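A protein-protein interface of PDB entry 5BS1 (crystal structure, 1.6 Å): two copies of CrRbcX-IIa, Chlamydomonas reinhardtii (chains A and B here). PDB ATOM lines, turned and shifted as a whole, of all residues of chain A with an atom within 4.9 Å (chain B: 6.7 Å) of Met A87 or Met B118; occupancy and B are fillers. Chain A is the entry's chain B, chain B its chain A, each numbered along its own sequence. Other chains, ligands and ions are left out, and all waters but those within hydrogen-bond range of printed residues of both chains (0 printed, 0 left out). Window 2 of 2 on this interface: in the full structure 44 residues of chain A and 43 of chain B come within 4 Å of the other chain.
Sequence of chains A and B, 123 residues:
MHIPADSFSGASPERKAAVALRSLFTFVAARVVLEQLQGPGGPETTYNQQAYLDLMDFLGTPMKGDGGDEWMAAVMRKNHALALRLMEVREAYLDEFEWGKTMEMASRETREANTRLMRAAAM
No position is printed for both chains.
The side-chain amide nitrogen (ND2) of Asn B114 is in hydrogen-bond range of the backbone carbonyl oxygen (O) of Met A87 (2.9 Å).
SD of Met A76 lies close to O of Leu B117, at 3.8 Å.
The side-chain carboxylate (OE1) of Glu A91 sits at hydrogen-bond distance from the side-chain amide nitrogen (ND2) of Asn B114, 3.0 Å away.
The side-chain amide oxygen (OD1) of Asn B114 sits at hydrogen-bond distance from the guanidinium group (NH2) of Arg A90.
Printed residues of chain B within 4 Å of Met A72: Leu B117.
Of chain B, only Asn B114 (2.9 Å), Leu B117 (3.5 Å) and Met B118 (3.6 Å) come within 4 Å of Met A87.
Val A89 touches none of the printed residues of chain B.
Of the printed residues of chain B, Arg A90 touches Ala B113 and Asn B114.
Of the printed residues of chain B, Glu A91 touches Asn B114 (3.0 Å).
Thr B110 touches none of the printed residues of chain A.
Printed residues of chain A within 4 Å of Ala B113: Arg A90 (3.7 Å).
Printed residues of chain A within 4 Å of Leu B117: Met A72 (3.5 Å), Met A76 (3.8 Å) and Met A87 (3.5 Å).
Met B118 touches just these residues of chain A: Leu A84 and Met A87.
The nearest residue of chain B that does not touch Met A87 is Ala B113 (5.0 Å).
The nearest residue of chain A that does not touch Met B118 is Met A76 (4.4 Å).
Among the printed residues, pairs that only touch across the chains: Leu A84 with Met B118 (3.2 Å), Met A72 with Leu B117 (3.5 Å), Met A87 with Leu B117 (3.5 Å), Met A87 with Met B118 (3.6 Å), Arg A90 with Ala B113 (3.7 Å) and Met A76 with Ala B121 (3.8 Å).
Hydrophobic or aromatic side chains of chain A that line the printed part of chain B: Met A72, Met A76, Leu A84 and Met A87.
Among the printed residues, no Asp or Glu carboxylate lies within 4 Å of a Lys or Arg side-chain nitrogen of the other chain.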
ATOM      1  N   MET A  72      -6.621   1.433 -18.884  1.00  0.00           N
ATOM      2  CA  MET A  72      -7.812   2.264 -18.787  1.00  0.00           C
ATOM      3  C   MET A  72      -8.194   2.825 -20.136  1.00  0.00           C
ATOM      4  O   MET A  72      -9.369   2.922 -20.452  1.00  0.00           O
ATOM      5  CB  MET A  72      -7.584   3.417 -17.797  1.00  0.00           C
ATOM      6  CG  MET A  72      -8.878   4.184 -17.507  1.00  0.00           C
ATOM      7  SD  MET A  72     -10.204   3.105 -16.566  1.00  0.00           S
ATOM      8  CE  MET A  72      -9.304   3.183 -14.834  1.00  0.00           C
ATOM      9  N   MET A  76     -11.715   2.348 -22.065  1.00  0.00           N
ATOM     10  CA  MET A  76     -12.497   3.486 -22.567  1.00  0.00           C
ATOM     11  C   MET A  76     -12.832   3.303 -24.028  1.00  0.00           C
ATOM     12  O   MET A  76     -13.930   3.662 -24.460  1.00  0.00           O
ATOM     13  CB  MET A  76     -11.800   4.822 -22.316  1.00  0.00           C
ATOM     14  CG  MET A  76     -12.748   5.995 -22.654  1.00  0.00           C
ATOM     15  SD  MET A  76     -11.823   7.638 -22.213  1.00  0.00           S
ATOM     16  CE  MET A  76     -12.895   8.161 -20.675  1.00  0.00           C
ATOM     17  N   ALA A  83     -15.414   2.926 -18.272  1.00  0.00           N
ATOM     18  CA  ALA A  83     -14.153   3.635 -17.969  1.00  0.00           C
ATOM     19  C   ALA A  83     -14.414   4.833 -17.059  1.00  0.00           C
ATOM     20  O   ALA A  83     -13.651   5.047 -16.109  1.00  0.00           O
ATOM     21  CB  ALA A  83     -13.450   4.082 -19.222  1.00  0.00           C
ATOM     22  N   LEU A  84     -15.473   5.596 -17.334  1.00  0.00           N
ATOM     23  CA  LEU A  84     -15.777   6.749 -16.477  1.00  0.00           C
ATOM     24  C   LEU A  84     -15.986   6.326 -15.037  1.00  0.00           C
ATOM     25  O   LEU A  84     -15.505   6.990 -14.113  1.00  0.00           O
ATOM     26  CB  LEU A  84     -17.005   7.528 -16.937  1.00  0.00           C
ATOM     27  CG  LEU A  84     -16.913   8.325 -18.240  1.00  0.00           C
ATOM     28  CD1 LEU A  84     -18.236   9.042 -18.440  1.00  0.00           C
ATOM     29  CD2 LEU A  84     -15.772   9.285 -18.270  1.00  0.00           C
ATOM     30  N   ARG A  85     -16.684   5.219 -14.845  1.00  0.00           N
ATOM     31  CA  ARG A  85     -16.958   4.734 -13.536  1.00  0.00           C
ATOM     32  C   ARG A  85     -15.668   4.245 -12.856  1.00  0.00           C
ATOM     33  O   ARG A  85     -15.437   4.566 -11.694  1.00  0.00           O
ATOM     34  CB  ARG A  85     -17.977   3.616 -13.578  1.00  0.00           C
ATOM     35  CG  ARG A  85     -18.295   3.006 -12.240  1.00  0.00           C
ATOM     36  CD  ARG A  85     -18.878   4.013 -11.254  1.00  0.00           C
ATOM     37  NE  ARG A  85     -19.168   3.365  -9.985  1.00  0.00           N
ATOM     38  CZ  ARG A  85     -19.226   3.991  -8.812  1.00  0.00           C
ATOM     39  NH1 ARG A  85     -19.010   5.296  -8.731  1.00  0.00           N
ATOM     40  NH2 ARG A  85     -19.491   3.299  -7.718  1.00  0.00           N
ATOM     41  N   LEU A  86     -14.836   3.512 -13.585  1.00  0.00           N
ATOM     42  CA  LEU A  86     -13.554   3.047 -13.016  1.00  0.00           C
ATOM     43  C   LEU A  86     -12.673   4.240 -12.630  1.00  0.00           C
ATOM     44  O   LEU A  86     -11.991   4.195 -11.612  1.00  0.00           O
ATOM     45  CB  LEU A  86     -12.833   2.152 -14.028  1.00  0.00           C
ATOM     46  CG  LEU A  86     -13.486   0.805 -14.295  1.00  0.00           C
ATOM     47  CD1 LEU A  86     -12.912   0.167 -15.567  1.00  0.00           C
ATOM     48  CD2 LEU A  86     -13.275  -0.124 -13.126  1.00  0.00           C
ATOM     49  N   MET A  87     -12.615   5.267 -13.487  1.00  0.00           N
ATOM     50  CA  MET A  87     -11.833   6.482 -13.212  1.00  0.00           C
ATOM     51  C   MET A  87     -12.329   7.174 -11.961  1.00  0.00           C
ATOM     52  O   MET A  87     -11.515   7.602 -11.129  1.00  0.00           O
ATOM     53  CB  MET A  87     -11.914   7.406 -14.430  1.00  0.00           C
ATOM     54  CG  MET A  87     -11.022   6.867 -15.536  1.00  0.00           C
ATOM     55  SD  MET A  87     -11.712   7.480 -17.291  1.00  0.00           S
ATOM     56  CE  MET A  87     -11.021   9.289 -17.207  1.00  0.00           C
ATOM     57  N   GLU A  88     -13.648   7.272 -11.805  1.00  0.00           N
ATOM     58  CA  GLU A  88     -14.251   7.916 -10.647  1.00  0.00           C
ATOM     59  C   GLU A  88     -13.838   7.191  -9.358  1.00  0.00           C
ATOM     60  O   GLU A  88     -13.465   7.823  -8.355  1.00  0.00           O
ATOM     61  CB  GLU A  88     -15.784   7.943 -10.810  1.00  0.00           C
ATOM     62  CG  GLU A  88     -16.591   8.382  -9.599  1.00  0.00           C
ATOM     63  CD  GLU A  88     -18.105   8.272  -9.745  1.00  0.00           C
ATOM     64  OE1 GLU A  88     -18.659   7.526 -10.604  1.00  0.00           O
ATOM     65  OE2 GLU A  88     -18.745   8.861  -8.853  1.00  0.00           O
ATOM     66  N   VAL A  89     -13.921   5.874  -9.400  1.00  0.00           N
ATOM     67  CA  VAL A  89     -13.692   5.058  -8.226  1.00  0.00           C
ATOM     68  C   VAL A  89     -12.218   5.076  -7.853  1.00  0.00           C
ATOM     69  O   VAL A  89     -11.895   5.214  -6.673  1.00  0.00           O
ATOM     70  CB  VAL A  89     -14.210   3.629  -8.444  1.00  0.00           C
ATOM     71  CG1 VAL A  89     -13.793   2.706  -7.327  1.00  0.00           C
ATOM     72  CG2 VAL A  89     -15.741   3.618  -8.559  1.00  0.00           C
ATOM     73  N   ARG A  90     -11.319   4.965  -8.831  1.00  0.00           N
ATOM     74  CA  ARG A  90      -9.894   4.984  -8.462  1.00  0.00           C
ATOM     75  C   ARG A  90      -9.457   6.346  -7.894  1.00  0.00           C
ATOM     76  O   ARG A  90      -8.605   6.399  -7.034  1.00  0.00           O
ATOM     77  CB  ARG A  90      -8.993   4.524  -9.608  1.00  0.00           C
ATOM     78  CG  ARG A  90      -8.763   5.529 -10.709  1.00  0.00           C
ATOM     79  CD  ARG A  90      -7.847   4.927 -11.778  1.00  0.00           C
ATOM     80  NE  ARG A  90      -7.605   5.860 -12.865  1.00  0.00           N
ATOM     81  CZ  ARG A  90      -6.701   5.674 -13.833  1.00  0.00           C
ATOM     82  NH1 ARG A  90      -5.942   4.588 -13.885  1.00  0.00           N
ATOM     83  NH2 ARG A  90      -6.548   6.607 -14.777  1.00  0.00           N
ATOM     84  N   GLU A  91     -10.074   7.439  -8.344  1.00  0.00           N
ATOM     85  CA  GLU A  91      -9.813   8.750  -7.787  1.00  0.00           C
ATOM     86  C   GLU A  91     -10.429   8.913  -6.389  1.00  0.00           C
ATOM     87  O   GLU A  91      -9.759   9.411  -5.463  1.00  0.00           O
ATOM     88  CB  GLU A  91     -10.327   9.830  -8.750  1.00  0.00           C
ATOM     89  CG  GLU A  91     -10.010  11.239  -8.262  1.00  0.00           C
ATOM     90  CD  GLU A  91     -10.065  12.320  -9.332  1.00  0.00           C
ATOM     91  OE1 GLU A  91      -9.980  12.023 -10.554  1.00  0.00           O
ATOM     92  OE2 GLU A  91     -10.156  13.510  -8.917  1.00  0.00           O
ATOM     93  N   THR B 110      -2.643  10.005 -10.525  1.00  0.00           N
ATOM     94  CA  THR B 110      -3.942   9.377 -10.747  1.00  0.00           C
ATOM     95  C   THR B 110      -4.944  10.409 -11.279  1.00  0.00           C
ATOM     96  O   THR B 110      -5.638  10.171 -12.278  1.00  0.00           O
ATOM     97  CB  THR B 110      -4.498   8.701  -9.498  1.00  0.00           C
ATOM     98  OG1 THR B 110      -3.635   7.609  -9.124  1.00  0.00           O
ATOM     99  CG2 THR B 110      -5.891   8.157  -9.739  1.00  0.00           C
ATOM    100  N   ALA B 113      -3.901  11.413 -14.825  1.00  0.00           N
ATOM    101  CA  ALA B 113      -4.232  10.403 -15.825  1.00  0.00           C
ATOM    102  C   ALA B 113      -5.722  10.439 -16.168  1.00  0.00           C
ATOM    103  O   ALA B 113      -6.095  10.317 -17.349  1.00  0.00           O
ATOM    104  CB  ALA B 113      -3.812   9.022 -15.355  1.00  0.00           C
ATOM    105  N   ASN B 114      -6.577  10.583 -15.156  1.00  0.00           N
ATOM    106  CA  ASN B 114      -8.009  10.679 -15.377  1.00  0.00           C
ATOM    107  C   ASN B 114      -8.294  11.903 -16.241  1.00  0.00           C
ATOM    108  O   ASN B 114      -9.053  11.827 -17.199  1.00  0.00           O
ATOM    109  CB  ASN B 114      -8.795  10.784 -14.072  1.00  0.00           C
ATOM    110  CG  ASN B 114      -8.944   9.466 -13.341  1.00  0.00           C
ATOM    111  OD1 ASN B 114      -8.528   8.420 -13.817  1.00  0.00           O
ATOM    112  ND2 ASN B 114      -9.553   9.519 -12.163  1.00  0.00           N
ATOM    113  N   THR B 115      -7.655  13.024 -15.929  1.00  0.00           N
ATOM    114  CA  THR B 115      -7.878  14.256 -16.720  1.00  0.00           C
ATOM    115  C   THR B 115      -7.457  14.091 -18.151  1.00  0.00           C
ATOM    116  O   THR B 115      -8.175  14.545 -19.054  1.00  0.00           O
ATOM    117  CB  THR B 115      -7.168  15.467 -16.075  1.00  0.00           C
ATOM    118  OG1 THR B 115      -7.762  15.687 -14.798  1.00  0.00           O
ATOM    119  CG2 THR B 115      -7.315  16.748 -16.945  1.00  0.00           C
ATOM    120  N   ARG B 116      -6.313  13.454 -18.383  1.00  0.00           N
ATOM    121  CA  ARG B 116      -5.829  13.202 -19.741  1.00  0.00           C
ATOM    122  C   ARG B 116      -6.861  12.392 -20.536  1.00  0.00           C
ATOM    123  O   ARG B 116      -7.204  12.744 -21.669  1.00  0.00           O
ATOM    124  CB  ARG B 116      -4.461  12.502 -19.746  1.00  0.00           C
ATOM    125  CG  ARG B 116      -3.314  13.486 -19.588  1.00  0.00           C
ATOM    126  CD  ARG B 116      -1.978  12.898 -20.049  1.00  0.00           C
ATOM    127  NE  ARG B 116      -1.768  11.518 -19.628  1.00  0.00           N
ATOM    128  CZ  ARG B 116      -1.308  11.118 -18.440  1.00  0.00           C
ATOM    129  NH1 ARG B 116      -1.166   9.816 -18.207  1.00  0.00           N
ATOM    130  NH2 ARG B 116      -1.006  11.980 -17.486  1.00  0.00           N
ATOM    131  N   LEU B 117      -7.370  11.330 -19.917  1.00  0.00           N
ATOM    132  CA  LEU B 117      -8.352  10.460 -20.566  1.00  0.00           C
ATOM    133  C   LEU B 117      -9.662  11.181 -20.834  1.00  0.00           C
ATOM    134  O   LEU B 117     -10.234  11.045 -21.903  1.00  0.00           O
ATOM    135  CB  LEU B 117      -8.579   9.196 -19.741  1.00  0.00           C
ATOM    136  CG  LEU B 117      -7.426   8.193 -19.825  1.00  0.00           C
ATOM    137  CD1 LEU B 117      -7.468   7.180 -18.687  1.00  0.00           C
ATOM    138  CD2 LEU B 117      -7.439   7.481 -21.171  1.00  0.00           C
ATOM    139  N   MET B 118     -10.106  11.992 -19.884  1.00  0.00           N
ATOM    140  CA  MET B 118     -11.324  12.785 -20.065  1.00  0.00           C
ATOM    141  C   MET B 118     -11.166  13.765 -21.209  1.00  0.00           C
ATOM    142  O   MET B 118     -12.070  13.904 -22.050  1.00  0.00           O
ATOM    143  CB  MET B 118     -11.634  13.529 -18.767  1.00  0.00           C
ATOM    144  CG  MET B 118     -12.189  12.654 -17.671  1.00  0.00           C
ATOM    145  SD  MET B 118     -13.806  11.780 -18.299  1.00  0.00           S
ATOM    146  CE  MET B 118     -14.997  13.340 -18.250  1.00  0.00           C
ATOM    147  N   ARG B 119     -10.019  14.432 -21.275  1.00  0.00           N
ATOM    148  CA  ARG B 119      -9.776  15.421 -22.335  1.00  0.00           C
ATOM    149  C   ARG B 119      -9.707  14.734 -23.703  1.00  0.00           C
ATOM    150  O   ARG B 119     -10.179  15.295 -24.707  1.00  0.00           O
ATOM    151  CB  ARG B 119      -8.533  16.288 -22.063  1.00  0.00           C
ATOM    152  CG  ARG B 119      -8.850  17.498 -21.187  1.00  0.00           C
ATOM    153  CD  ARG B 119      -7.666  18.345 -20.726  1.00  0.00           C
ATOM    154  NE  ARG B 119      -8.029  19.140 -19.545  1.00  0.00           N
ATOM    155  CZ  ARG B 119      -8.650  20.327 -19.560  1.00  0.00           C
ATOM    156  NH1 ARG B 119      -8.991  20.925 -20.703  1.00  0.00           N
ATOM    157  NH2 ARG B 119      -8.921  20.937 -18.408  1.00  0.00           N
ATOM    158  N   ALA B 120      -9.181  13.516 -23.740  1.00  0.00           N
ATOM    159  CA  ALA B 120      -9.073  12.758 -24.978  1.00  0.00           C
ATOM    160  C   ALA B 120     -10.442  12.336 -25.518  1.00  0.00           C
ATOM    161  O   ALA B 120     -10.640  12.300 -26.734  1.00  0.00           O
ATOM    162  CB  ALA B 120      -8.194  11.540 -24.782  1.00  0.00           C
ATOM    163  N   ALA B 121     -11.386  12.018 -24.642  1.00  0.00           N
ATOM    164  CA  ALA B 121     -12.707  11.542 -25.079  1.00  0.00           C
ATOM    165  C   ALA B 121     -13.661  12.693 -25.280  1.00  0.00           C
ATOM    166  O   ALA B 121     -14.777  12.500 -25.760  1.00  0.00           O
ATOM    167  CB  ALA B 121     -13.285  10.555 -24.078  1.00  0.00           C
ATOM    168  N   ALA B 122     -13.205  13.899 -24.952  1.00  0.00           N
ATOM    169  CA  ALA B 122     -14.051  15.083 -25.012  1.00  0.00           C
ATOM    170  C   ALA B 122     -14.429  15.480 -26.454  1.00  0.00           C
ATOM    171  O   ALA B 122     -15.402  16.205 -26.645  1.00  0.00           O
ATOM    172  CB  ALA B 122     -13.403  16.237 -24.242  1.00  0.00           C
ATOM    173  N   MET B 123     -13.661  15.019 -27.445  1.00  0.00           N
ATOM    174  CA  MET B 123     -14.127  14.880 -28.852  1.00  0.00           C
ATOM    175  C   MET B 123     -13.362  15.817 -29.768  1.00  0.00           C
ATOM    176  O   MET B 123     -12.130  15.853 -29.665  1.00  0.00           O
ATOM    177  OXT MET B 123     -13.874  16.520 -30.655  1.00  0.00           O
ATOM    178  CB  MET B 123     -15.673  14.943 -29.072  1.00  0.00           C
ATOM    179  CG  MET B 123     -16.157  13.615 -29.656  1.00  0.00           C
ATOM    180  SD  MET B 123     -18.134  13.411 -29.526  1.00  0.00           S
ATOM    181  CE  MET B 123     -17.918  12.093 -28.111  1.00  0.00           C
